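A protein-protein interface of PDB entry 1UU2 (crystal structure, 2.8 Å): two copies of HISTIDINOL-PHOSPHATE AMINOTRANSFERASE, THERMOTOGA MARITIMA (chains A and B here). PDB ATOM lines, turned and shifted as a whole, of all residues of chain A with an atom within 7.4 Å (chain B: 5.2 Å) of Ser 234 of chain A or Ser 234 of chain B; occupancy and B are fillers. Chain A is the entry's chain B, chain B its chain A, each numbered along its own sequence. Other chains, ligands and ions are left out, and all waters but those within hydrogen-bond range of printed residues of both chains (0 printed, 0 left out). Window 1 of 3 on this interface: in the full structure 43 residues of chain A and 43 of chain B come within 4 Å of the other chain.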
ATOM      1  N   TYR A  54      12.637  26.577 -13.425  1.00  0.00           N
ATOM      2  CA  TYR A  54      13.943  26.428 -14.050  1.00  0.00           C
ATOM      3  C   TYR A  54      14.003  25.392 -15.166  1.00  0.00           C
ATOM      4  O   TYR A  54      13.578  24.249 -14.992  1.00  0.00           O
ATOM      5  CB  TYR A  54      14.977  26.080 -12.986  1.00  0.00           C
ATOM      6  CG  TYR A  54      16.383  26.335 -13.455  1.00  0.00           C
ATOM      7  CD1 TYR A  54      16.793  27.622 -13.771  1.00  0.00           C
ATOM      8  CD2 TYR A  54      17.282  25.289 -13.614  1.00  0.00           C
ATOM      9  CE1 TYR A  54      18.076  27.866 -14.242  1.00  0.00           C
ATOM     10  CE2 TYR A  54      18.575  25.528 -14.091  1.00  0.00           C
ATOM     11  CZ  TYR A  54      18.960  26.820 -14.401  1.00  0.00           C
ATOM     12  OH  TYR A  54      20.224  27.077 -14.865  1.00  0.00           O
ATOM     13  N   ASP A  55      14.554  25.807 -16.305  1.00  0.00           N
ATOM     14  CA  ASP A  55      14.689  24.936 -17.472  1.00  0.00           C
ATOM     15  C   ASP A  55      15.199  23.575 -17.046  1.00  0.00           C
ATOM     16  O   ASP A  55      16.243  23.486 -16.408  1.00  0.00           O
ATOM     17  CB  ASP A  55      15.674  25.546 -18.465  1.00  0.00           C
ATOM     18  CG  ASP A  55      15.157  26.831 -19.090  1.00  0.00           C
ATOM     19  OD1 ASP A  55      15.918  27.449 -19.862  1.00  0.00           O
ATOM     20  OD2 ASP A  55      13.999  27.214 -18.813  1.00  0.00           O
ATOM     21  N   SER A  56      14.461  22.521 -17.389  1.00  0.00           N
ATOM     22  CA  SER A  56      14.862  21.164 -17.026  1.00  0.00           C
ATOM     23  C   SER A  56      16.305  20.946 -17.497  1.00  0.00           C
ATOM     24  O   SER A  56      17.238  21.328 -16.787  1.00  0.00           O
ATOM     25  CB  SER A  56      13.903  20.144 -17.639  1.00  0.00           C
ATOM     26  OG  SER A  56      14.238  18.837 -17.217  1.00  0.00           O
ATOM     27  N   LEU A  61      24.365  22.784 -18.579  1.00  0.00           N
ATOM     28  CA  LEU A  61      24.487  21.407 -18.128  1.00  0.00           C
ATOM     29  C   LEU A  61      24.711  20.435 -19.285  1.00  0.00           C
ATOM     30  O   LEU A  61      25.613  19.597 -19.234  1.00  0.00           O
ATOM     31  CB  LEU A  61      23.233  21.027 -17.341  1.00  0.00           C
ATOM     32  CG  LEU A  61      23.311  19.826 -16.398  1.00  0.00           C
ATOM     33  CD1 LEU A  61      22.439  20.079 -15.180  1.00  0.00           C
ATOM     34  CD2 LEU A  61      22.886  18.570 -17.123  1.00  0.00           C
ATOM     35  N   ASN A  83      14.992  12.729 -13.658  1.00  0.00           N
ATOM     36  CA  ASN A  83      15.031  12.715 -12.200  1.00  0.00           C
ATOM     37  C   ASN A  83      15.638  11.391 -11.767  1.00  0.00           C
ATOM     38  O   ASN A  83      14.930  10.447 -11.415  1.00  0.00           O
ATOM     39  CB  ASN A  83      13.615  12.869 -11.634  1.00  0.00           C
ATOM     40  CG  ASN A  83      13.571  12.742 -10.121  1.00  0.00           C
ATOM     41  OD1 ASN A  83      14.474  13.202  -9.420  1.00  0.00           O
ATOM     42  ND2 ASN A  83      12.507  12.129  -9.608  1.00  0.00           N
ATOM     43  N   LEU A 206      26.282  11.544  -5.819  1.00  0.00           N
ATOM     44  CA  LEU A 206      25.136  12.446  -5.818  1.00  0.00           C
ATOM     45  C   LEU A 206      23.819  11.684  -5.798  1.00  0.00           C
ATOM     46  O   LEU A 206      22.764  12.233  -6.120  1.00  0.00           O
ATOM     47  CB  LEU A 206      25.186  13.352  -7.045  1.00  0.00           C
ATOM     48  CG  LEU A 206      25.870  14.714  -6.908  1.00  0.00           C
ATOM     49  CD1 LEU A 206      26.469  14.877  -5.521  1.00  0.00           C
ATOM     50  CD2 LEU A 206      26.931  14.850  -7.989  1.00  0.00           C
ATOM     51  N   ALA A 207      23.889  10.417  -5.411  1.00  0.00           N
ATOM     52  CA  ALA A 207      22.714   9.556  -5.351  1.00  0.00           C
ATOM     53  C   ALA A 207      21.517  10.212  -4.663  1.00  0.00           C
ATOM     54  O   ALA A 207      20.371   9.853  -4.929  1.00  0.00           O
ATOM     55  CB  ALA A 207      23.067   8.249  -4.641  1.00  0.00           C
ATOM     56  N   ALA A 208      21.776  11.169  -3.781  1.00  0.00           N
ATOM     57  CA  ALA A 208      20.693  11.831  -3.070  1.00  0.00           C
ATOM     58  C   ALA A 208      20.058  12.968  -3.868  1.00  0.00           C
ATOM     59  O   ALA A 208      18.931  13.376  -3.586  1.00  0.00           O
ATOM     60  CB  ALA A 208      21.197  12.348  -1.731  1.00  0.00           C
ATOM     61  N   GLN A 209      20.766  13.468  -4.874  1.00  0.00           N
ATOM     62  CA  GLN A 209      20.239  14.570  -5.668  1.00  0.00           C
ATOM     63  C   GLN A 209      19.596  14.184  -6.996  1.00  0.00           C
ATOM     64  O   GLN A 209      19.257  15.051  -7.799  1.00  0.00           O
ATOM     65  CB  GLN A 209      21.331  15.611  -5.892  1.00  0.00           C
ATOM     66  CG  GLN A 209      21.713  16.298  -4.608  1.00  0.00           C
ATOM     67  CD  GLN A 209      20.513  16.926  -3.919  1.00  0.00           C
ATOM     68  OE1 GLN A 209      19.953  17.915  -4.400  1.00  0.00           O
ATOM     69  NE2 GLN A 209      20.102  16.347  -2.795  1.00  0.00           N
ATOM     70  N   ARG A 210      19.431  12.882  -7.212  1.00  0.00           N
ATOM     71  CA  ARG A 210      18.798  12.340  -8.415  1.00  0.00           C
ATOM     72  C   ARG A 210      19.089  13.104  -9.698  1.00  0.00           C
ATOM     73  O   ARG A 210      18.372  14.047 -10.030  1.00  0.00           O
ATOM     74  CB  ARG A 210      17.276  12.298  -8.227  1.00  0.00           C
ATOM     75  CG  ARG A 210      16.816  12.002  -6.805  1.00  0.00           C
ATOM     76  CD  ARG A 210      17.294  10.644  -6.339  1.00  0.00           C
ATOM     77  NE  ARG A 210      16.756   9.557  -7.154  1.00  0.00           N
ATOM     78  CZ  ARG A 210      17.498   8.630  -7.754  1.00  0.00           C
ATOM     79  NH1 ARG A 210      16.920   7.680  -8.471  1.00  0.00           N
ATOM     80  NH2 ARG A 210      18.820   8.656  -7.644  1.00  0.00           N
ATOM     81  N   VAL A 211      20.119  12.709 -10.434  1.00  0.00           N
ATOM     82  CA  VAL A 211      20.416  13.393 -11.684  1.00  0.00           C
ATOM     83  C   VAL A 211      20.951  12.430 -12.738  1.00  0.00           C
ATOM     84  O   VAL A 211      22.101  12.008 -12.680  1.00  0.00           O
ATOM     85  CB  VAL A 211      21.440  14.528 -11.483  1.00  0.00           C
ATOM     86  CG1 VAL A 211      21.532  15.352 -12.748  1.00  0.00           C
ATOM     87  N   PHE A 231       9.417  19.670 -15.762  1.00  0.00           N
ATOM     88  CA  PHE A 231      10.458  20.115 -14.840  1.00  0.00           C
ATOM     89  C   PHE A 231      10.717  18.999 -13.838  1.00  0.00           C
ATOM     90  O   PHE A 231      10.135  18.973 -12.750  1.00  0.00           O
ATOM     91  CB  PHE A 231      10.017  21.379 -14.097  1.00  0.00           C
ATOM     92  CG  PHE A 231       9.445  22.437 -14.990  1.00  0.00           C
ATOM     93  CD1 PHE A 231       8.072  22.558 -15.149  1.00  0.00           C
ATOM     94  CD2 PHE A 231      10.281  23.298 -15.691  1.00  0.00           C
ATOM     95  CE1 PHE A 231       7.538  23.520 -15.995  1.00  0.00           C
ATOM     96  CE2 PHE A 231       9.756  24.265 -16.541  1.00  0.00           C
ATOM     97  CZ  PHE A 231       8.382  24.376 -16.694  1.00  0.00           C
ATOM     98  N   ASN A 232      11.600  18.084 -14.209  1.00  0.00           N
ATOM     99  CA  ASN A 232      11.908  16.940 -13.374  1.00  0.00           C
ATOM    100  C   ASN A 232      13.209  17.030 -12.599  1.00  0.00           C
ATOM    101  O   ASN A 232      13.393  16.315 -11.614  1.00  0.00           O
ATOM    102  CB  ASN A 232      11.907  15.671 -14.231  1.00  0.00           C
ATOM    103  CG  ASN A 232      12.719  15.821 -15.509  1.00  0.00           C
ATOM    104  OD1 ASN A 232      12.842  14.876 -16.283  1.00  0.00           O
ATOM    105  ND2 ASN A 232      13.270  17.006 -15.736  1.00  0.00           N
ATOM    106  N   VAL A 233      14.109  17.902 -13.036  1.00  0.00           N
ATOM    107  CA  VAL A 233      15.392  18.045 -12.365  1.00  0.00           C
ATOM    108  C   VAL A 233      15.579  19.427 -11.751  1.00  0.00           C
ATOM    109  O   VAL A 233      15.787  20.411 -12.455  1.00  0.00           O
ATOM    110  CB  VAL A 233      16.536  17.736 -13.339  1.00  0.00           C
ATOM    111  CG1 VAL A 233      16.397  16.312 -13.832  1.00  0.00           C
ATOM    112  CG2 VAL A 233      16.492  18.692 -14.519  1.00  0.00           C
ATOM    113  N   SER A 234      15.506  19.481 -10.424  1.00  0.00           N
ATOM    114  CA  SER A 234      15.642  20.726  -9.668  1.00  0.00           C
ATOM    115  C   SER A 234      16.830  21.616 -10.041  1.00  0.00           C
ATOM    116  O   SER A 234      17.816  21.173 -10.630  1.00  0.00           O
ATOM    117  CB  SER A 234      15.698  20.420  -8.167  1.00  0.00           C
ATOM    118  OG  SER A 234      16.788  19.571  -7.860  1.00  0.00           O
ATOM    119  N   TYR A 235      16.712  22.885  -9.676  1.00  0.00           N
ATOM    120  CA  TYR A 235      17.738  23.882  -9.938  1.00  0.00           C
ATOM    121  C   TYR A 235      19.025  23.551  -9.184  1.00  0.00           C
ATOM    122  O   TYR A 235      20.117  23.586  -9.754  1.00  0.00           O
ATOM    123  CB  TYR A 235      17.200  25.254  -9.523  1.00  0.00           C
ATOM    124  CG  TYR A 235      18.201  26.387  -9.523  1.00  0.00           C
ATOM    125  CD1 TYR A 235      18.994  26.652 -10.640  1.00  0.00           C
ATOM    126  CD2 TYR A 235      18.323  27.227  -8.413  1.00  0.00           C
ATOM    127  CE1 TYR A 235      19.877  27.725 -10.653  1.00  0.00           C
ATOM    128  CE2 TYR A 235      19.203  28.303  -8.417  1.00  0.00           C
ATOM    129  CZ  TYR A 235      19.976  28.545  -9.541  1.00  0.00           C
ATOM    130  OH  TYR A 235      20.841  29.611  -9.553  1.00  0.00           O
ATOM    131  N   VAL A 236      18.884  23.220  -7.906  1.00  0.00           N
ATOM    132  CA  VAL A 236      20.030  22.881  -7.074  1.00  0.00           C
ATOM    133  C   VAL A 236      20.697  21.579  -7.514  1.00  0.00           C
ATOM    134  O   VAL A 236      21.926  21.472  -7.517  1.00  0.00           O
ATOM    135  CB  VAL A 236      19.623  22.762  -5.598  1.00  0.00           C
ATOM    136  CG1 VAL A 236      20.815  22.313  -4.763  1.00  0.00           C
ATOM    137  CG2 VAL A 236      19.105  24.100  -5.107  1.00  0.00           C
ATOM    138  N   SER A 237      19.887  20.591  -7.881  1.00  0.00           N
ATOM    139  CA  SER A 237      20.427  19.319  -8.332  1.00  0.00           C
ATOM    140  C   SER A 237      21.249  19.556  -9.582  1.00  0.00           C
ATOM    141  O   SER A 237      22.340  19.019  -9.729  1.00  0.00           O
ATOM    142  CB  SER A 237      19.305  18.332  -8.647  1.00  0.00           C
ATOM    143  OG  SER A 237      18.627  17.932  -7.471  1.00  0.00           O
ATOM    144  N   GLN A 238      20.723  20.376 -10.481  1.00  0.00           N
ATOM    145  CA  GLN A 238      21.419  20.663 -11.722  1.00  0.00           C
ATOM    146  C   GLN A 238      22.750  21.358 -11.495  1.00  0.00           C
ATOM    147  O   GLN A 238      23.659  21.239 -12.313  1.00  0.00           O
ATOM    148  CB  GLN A 238      20.536  21.507 -12.646  1.00  0.00           C
ATOM    149  CG  GLN A 238      19.345  20.743 -13.209  1.00  0.00           C
ATOM    150  CD  GLN A 238      18.769  21.387 -14.456  1.00  0.00           C
ATOM    151  OE1 GLN A 238      17.630  21.855 -14.461  1.00  0.00           O
ATOM    152  NE2 GLN A 238      19.555  21.412 -15.521  1.00  0.00           N
ATOM    153  N   MET A 239      22.877  22.077 -10.386  1.00  0.00           N
ATOM    154  CA  MET A 239      24.126  22.772 -10.105  1.00  0.00           C
ATOM    155  C   MET A 239      25.185  21.751  -9.706  1.00  0.00           C
ATOM    156  O   MET A 239      26.319  21.800 -10.183  1.00  0.00           O
ATOM    157  CB  MET A 239      23.930  23.790  -8.984  1.00  0.00           C
ATOM    158  CG  MET A 239      24.985  24.897  -8.954  1.00  0.00           C
ATOM    159  SD  MET A 239      24.953  25.968 -10.418  1.00  0.00           S
ATOM    160  CE  MET A 239      23.716  27.185  -9.926  1.00  0.00           C
ATOM    161  N   PHE A 240      24.801  20.822  -8.836  1.00  0.00           N
ATOM    162  CA  PHE A 240      25.705  19.773  -8.381  1.00  0.00           C
ATOM    163  C   PHE A 240      26.332  18.985  -9.526  1.00  0.00           C
ATOM    164  O   PHE A 240      27.521  18.657  -9.482  1.00  0.00           O
ATOM    165  CB  PHE A 240      24.967  18.814  -7.453  1.00  0.00           C
ATOM    166  CG  PHE A 240      24.945  19.263  -6.039  1.00  0.00           C
ATOM    167  CD1 PHE A 240      26.113  19.266  -5.288  1.00  0.00           C
ATOM    168  CD2 PHE A 240      23.773  19.735  -5.464  1.00  0.00           C
ATOM    169  CE1 PHE A 240      26.117  19.737  -3.987  1.00  0.00           C
ATOM    170  CE2 PHE A 240      23.764  20.208  -4.165  1.00  0.00           C
ATOM    171  CZ  PHE A 240      24.938  20.210  -3.424  1.00  0.00           C
ATOM    172  N   ALA B 208      11.481  26.024  -8.327  1.00  0.00           N
ATOM    173  CA  ALA B 208      12.667  25.492  -8.979  1.00  0.00           C
ATOM    174  C   ALA B 208      13.172  24.220  -8.312  1.00  0.00           C
ATOM    175  O   ALA B 208      14.051  23.543  -8.848  1.00  0.00           O
ATOM    176  CB  ALA B 208      13.761  26.537  -8.986  1.00  0.00           C
ATOM    177  N   GLN B 209      12.613  23.894  -7.148  1.00  0.00           N
ATOM    178  CA  GLN B 209      13.032  22.704  -6.422  1.00  0.00           C
ATOM    179  C   GLN B 209      12.030  21.559  -6.444  1.00  0.00           C
ATOM    180  O   GLN B 209      12.201  20.559  -5.750  1.00  0.00           O
ATOM    181  CB  GLN B 209      13.391  23.068  -4.984  1.00  0.00           C
ATOM    182  CG  GLN B 209      14.717  23.792  -4.889  1.00  0.00           C
ATOM    183  CD  GLN B 209      15.821  23.057  -5.626  1.00  0.00           C
ATOM    184  OE1 GLN B 209      16.198  21.947  -5.261  1.00  0.00           O
ATOM    185  NE2 GLN B 209      16.340  23.675  -6.672  1.00  0.00           N
ATOM    186  N   ARG B 210      10.981  21.723  -7.237  1.00  0.00           N
ATOM    187  CA  ARG B 210       9.955  20.699  -7.416  1.00  0.00           C
ATOM    188  C   ARG B 210       9.592  19.827  -6.201  1.00  0.00           C
ATOM    189  O   ARG B 210      10.078  18.700  -6.073  1.00  0.00           O
ATOM    190  CB  ARG B 210      10.382  19.788  -8.567  1.00  0.00           C
ATOM    191  CG  ARG B 210      11.217  20.488  -9.642  1.00  0.00           C
ATOM    192  CD  ARG B 210      10.427  21.551 -10.392  1.00  0.00           C
ATOM    193  NE  ARG B 210       9.248  20.979 -11.037  1.00  0.00           N
ATOM    194  CZ  ARG B 210       7.999  21.180 -10.630  1.00  0.00           C
ATOM    195  NH1 ARG B 210       7.749  21.947  -9.579  1.00  0.00           N
ATOM    196  NH2 ARG B 210       6.996  20.600 -11.270  1.00  0.00           N
ATOM    197  N   ASN B 232      12.172  10.212  -5.637  1.00  0.00           N
ATOM    198  CA  ASN B 232      11.754  11.285  -6.529  1.00  0.00           C
ATOM    199  C   ASN B 232      12.078  12.710  -6.062  1.00  0.00           C
ATOM    200  O   ASN B 232      12.221  13.625  -6.884  1.00  0.00           O
ATOM    201  CB  ASN B 232      10.247  11.151  -6.808  1.00  0.00           C
ATOM    202  CG  ASN B 232       9.426  10.940  -5.542  1.00  0.00           C
ATOM    203  OD1 ASN B 232       8.205  10.805  -5.601  1.00  0.00           O
ATOM    204  ND2 ASN B 232      10.091  10.907  -4.392  1.00  0.00           N
ATOM    205  N   VAL B 233      12.192  12.902  -4.752  1.00  0.00           N
ATOM    206  CA  VAL B 233      12.497  14.224  -4.212  1.00  0.00           C
ATOM    207  C   VAL B 233      13.902  14.218  -3.635  1.00  0.00           C
ATOM    208  O   VAL B 233      14.191  13.479  -2.695  1.00  0.00           O
ATOM    209  CB  VAL B 233      11.499  14.630  -3.100  1.00  0.00           C
ATOM    210  CG1 VAL B 233      11.832  16.021  -2.599  1.00  0.00           C
ATOM    211  CG2 VAL B 233      10.066  14.590  -3.630  1.00  0.00           C
ATOM    212  N   SER B 234      14.772  15.046  -4.199  1.00  0.00           N
ATOM    213  CA  SER B 234      16.156  15.115  -3.751  1.00  0.00           C
ATOM    214  C   SER B 234      16.321  15.546  -2.298  1.00  0.00           C
ATOM    215  O   SER B 234      15.443  16.185  -1.721  1.00  0.00           O
ATOM    216  CB  SER B 234      16.961  16.047  -4.664  1.00  0.00           C
ATOM    217  OG  SER B 234      16.402  17.348  -4.719  1.00  0.00           O
ATOM    218  N   TYR B 235      17.462  15.174  -1.721  1.00  0.00           N
ATOM    219  CA  TYR B 235      17.802  15.499  -0.340  1.00  0.00           C
ATOM    220  C   TYR B 235      17.677  16.998  -0.113  1.00  0.00           C
ATOM    221  O   TYR B 235      16.921  17.446   0.751  1.00  0.00           O
ATOM    222  CB  TYR B 235      19.233  15.044  -0.051  1.00  0.00           C
ATOM    223  CG  TYR B 235      19.777  15.449   1.302  1.00  0.00           C
ATOM    224  CD1 TYR B 235      19.221  14.952   2.479  1.00  0.00           C
ATOM    225  CD2 TYR B 235      20.864  16.317   1.402  1.00  0.00           C
ATOM    226  CE1 TYR B 235      19.735  15.307   3.722  1.00  0.00           C
ATOM    227  CE2 TYR B 235      21.386  16.677   2.640  1.00  0.00           C
ATOM    228  CZ  TYR B 235      20.818  16.168   3.797  1.00  0.00           C
ATOM    229  OH  TYR B 235      21.340  16.512   5.025  1.00  0.00           O
ATOM    230  N   VAL B 236      18.420  17.774  -0.895  1.00  0.00           N
ATOM    231  CA  VAL B 236      18.377  19.224  -0.780  1.00  0.00           C
ATOM    232  C   VAL B 236      16.968  19.776  -1.006  1.00  0.00           C
ATOM    233  O   VAL B 236      16.576  20.749  -0.375  1.00  0.00           O
ATOM    234  CB  VAL B 236      19.344  19.883  -1.779  1.00  0.00           C
ATOM    235  CG1 VAL B 236      19.276  21.386  -1.651  1.00  0.00           C
ATOM    236  CG2 VAL B 236      20.760  19.393  -1.522  1.00  0.00           C
ATOM    237  N   SER B 237      16.207  19.163  -1.906  1.00  0.00           N
ATOM    238  CA  SER B 237      14.845  19.614  -2.167  1.00  0.00           C
ATOM    239  C   SER B 237      14.010  19.523  -0.895  1.00  0.00           C
ATOM    240  O   SER B 237      13.282  20.451  -0.547  1.00  0.00           O
ATOM    241  CB  SER B 237      14.185  18.764  -3.255  1.00  0.00           C
ATOM    242  OG  SER B 237      14.792  18.968  -4.516  1.00  0.00           O
ATOM    243  N   GLN B 238      14.111  18.397  -0.202  1.00  0.00           N
ATOM    244  CA  GLN B 238      13.361  18.222   1.026  1.00  0.00           C
ATOM    245  C   GLN B 238      13.880  19.220   2.047  1.00  0.00           C
ATOM    246  O   GLN B 238      13.109  19.814   2.804  1.00  0.00           O
ATOM    247  CB  GLN B 238      13.535  16.806   1.560  1.00  0.00           C
ATOM    248  CG  GLN B 238      13.305  15.727   0.528  1.00  0.00           C
ATOM    249  CD  GLN B 238      13.269  14.347   1.144  1.00  0.00           C
ATOM    250  OE1 GLN B 238      13.376  13.336   0.449  1.00  0.00           O
ATOM    251  NE2 GLN B 238      13.110  14.297   2.458  1.00  0.00           N
ATOM    252  N   MET B 239      15.196  19.400   2.057  1.00  0.00           N
ATOM    253  CA  MET B 239      15.829  20.327   2.980  1.00  0.00           C
ATOM    254  C   MET B 239      15.207  21.717   2.827  1.00  0.00           C
ATOM    255  O   MET B 239      14.852  22.359   3.817  1.00  0.00           O
ATOM    256  CB  MET B 239      17.337  20.379   2.709  1.00  0.00           C
ATOM    257  CG  MET B 239      18.163  21.004   3.831  1.00  0.00           C
ATOM    258  SD  MET B 239      17.894  20.215   5.446  1.00  0.00           S
ATOM    259  CE  MET B 239      18.726  18.621   5.201  1.00  0.00           C
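The side-chain amide nitrogen of Gln 209 of chain B sits close to the backbone NH of Tyr 235 of chain A.
The backbone carbonyl oxygen (O) of Phe 231 of chain A sits at hydrogen-bond distance from the guanidinium group (NE) of Arg 210 of chain B (2.8 Å).
The backbone NH (N) of Tyr 235 of chain B lies close to the side-chain amide nitrogen (NE2) of Gln 209 of chain A (3.1 Å).
The backbone NH (N) of Val 236 of chain A sits close to the side-chain amide nitrogen (NE2) of Gln 209 of chain B (2.9 Å).
N of Tyr 235 of chain B sits at hydrogen-bond distance from O of Ala 208 of chain A.
N of Tyr 235 of chain A is in hydrogen-bond range of O of Ala 208 of chain B (2.9 Å).
The backbone carbonyl oxygen (O) of Asn 232 of chain B is in hydrogen-bond range of the side-chain amide nitrogen (ND2) of Asn 83 of chain A (3.1 Å).
NE2 of Gln 209 of chain A sits close to N of Val 236 of chain B (2.9 Å).
O of Gln 209 of chain B is in hydrogen-bond range of OG of Ser 237 of chain B, 3.3 Å away.
The side-chain hydroxyl of Ser 234 of chain A lies within hydrogen-bond range of the side-chain hydroxyl of Ser 237 of chain A (2.5 Å).
The backbone NH of Ser 237 of chain B sits close to the side-chain hydroxyl of Ser 234 of chain B (3.4 Å).
OG of Ser 237 of chain A sits at hydrogen-bond distance from O of Gln 209 of chain A (3.0 Å).
Ala 208 of chain A touches Ser 234 of chain B.
Gln 209 of chain A touches Ser 234 of chain B (OE1 to CB, 3.5 Å).
Ala 208 of chain B touches Ser 234 of chain A.
Ser 234 of chain A touches Gln 209 of chain B (CB to OE1, 3.3 Å).
Ser 234 of chain A touches Ser 234 of chain B (OG to OG, 3.9 Å).
Ser 234 of chain A touches Ser 237 of chain B (OG to OG, 3.9 Å).
Val 236 of chain A touches Val 236 of chain B.
Ser 234 of chain B touches Ser 237 of chain A.
Printed residues of chain B within 4 Å of Asn 83 of chain A: Asn 232.
Of the printed residues of chain B, Ser 234 of chain A touches Ala 208, Gln 209, Ser 234 and Ser 237.
Printed residues of chain A within 4 Å of Ala 208 of chain B: Ser 234 (3.3 Å) and Tyr 235 (2.9 Å).
Printed residues of chain A within 4 Å of Arg 210 of chain B: Phe 231.
Ser 234 of chain B touches just these residues of chain A: Ala 208 (3.3 Å), Gln 209 (3.5 Å), Ser 234 (3.9 Å) and Ser 237 (3.6 Å).
The nearest residue of chain B that does not touch Ser 234 of chain A is Arg 210 of chain B (4.4 Å).
The nearest residue of chain A that does not touch Ser 234 of chain B is Arg 210 of chain A (4.4 Å).
Hydrophobic or aromatic side chains of chain B that line the printed part of chain A: Ala 208, Tyr 235 and Val 236.
Of the 21 printed residues of chain A, 8 touch a printed residue of chain B.
Among the printed residues, no Asp or Glu carboxylate lies within 4 Å of a Lys or Arg side-chain nitrogen of the other chain.
Ala 208 of chain A touches Tyr 235 of chain B, and with the chains exchanged Tyr 235 of chain A touches Ala 208 of chain B.
Gln 209 of chain A touches Ser 234 of chain B, and with the chains exchanged Ser 234 of chain A touches Gln 209 of chain B.
Gln 209 of chain A touches Tyr 235 of chain B, and with the chains exchanged Tyr 235 of chain A touches Gln 209 of chain B.
Ser 234 of chain B touches its own counterpart, Ser 234 of chain A.
Of the 16 pairs that touch across the chains among the printed residues, 14 have their exchanged pair printed and touching as well.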
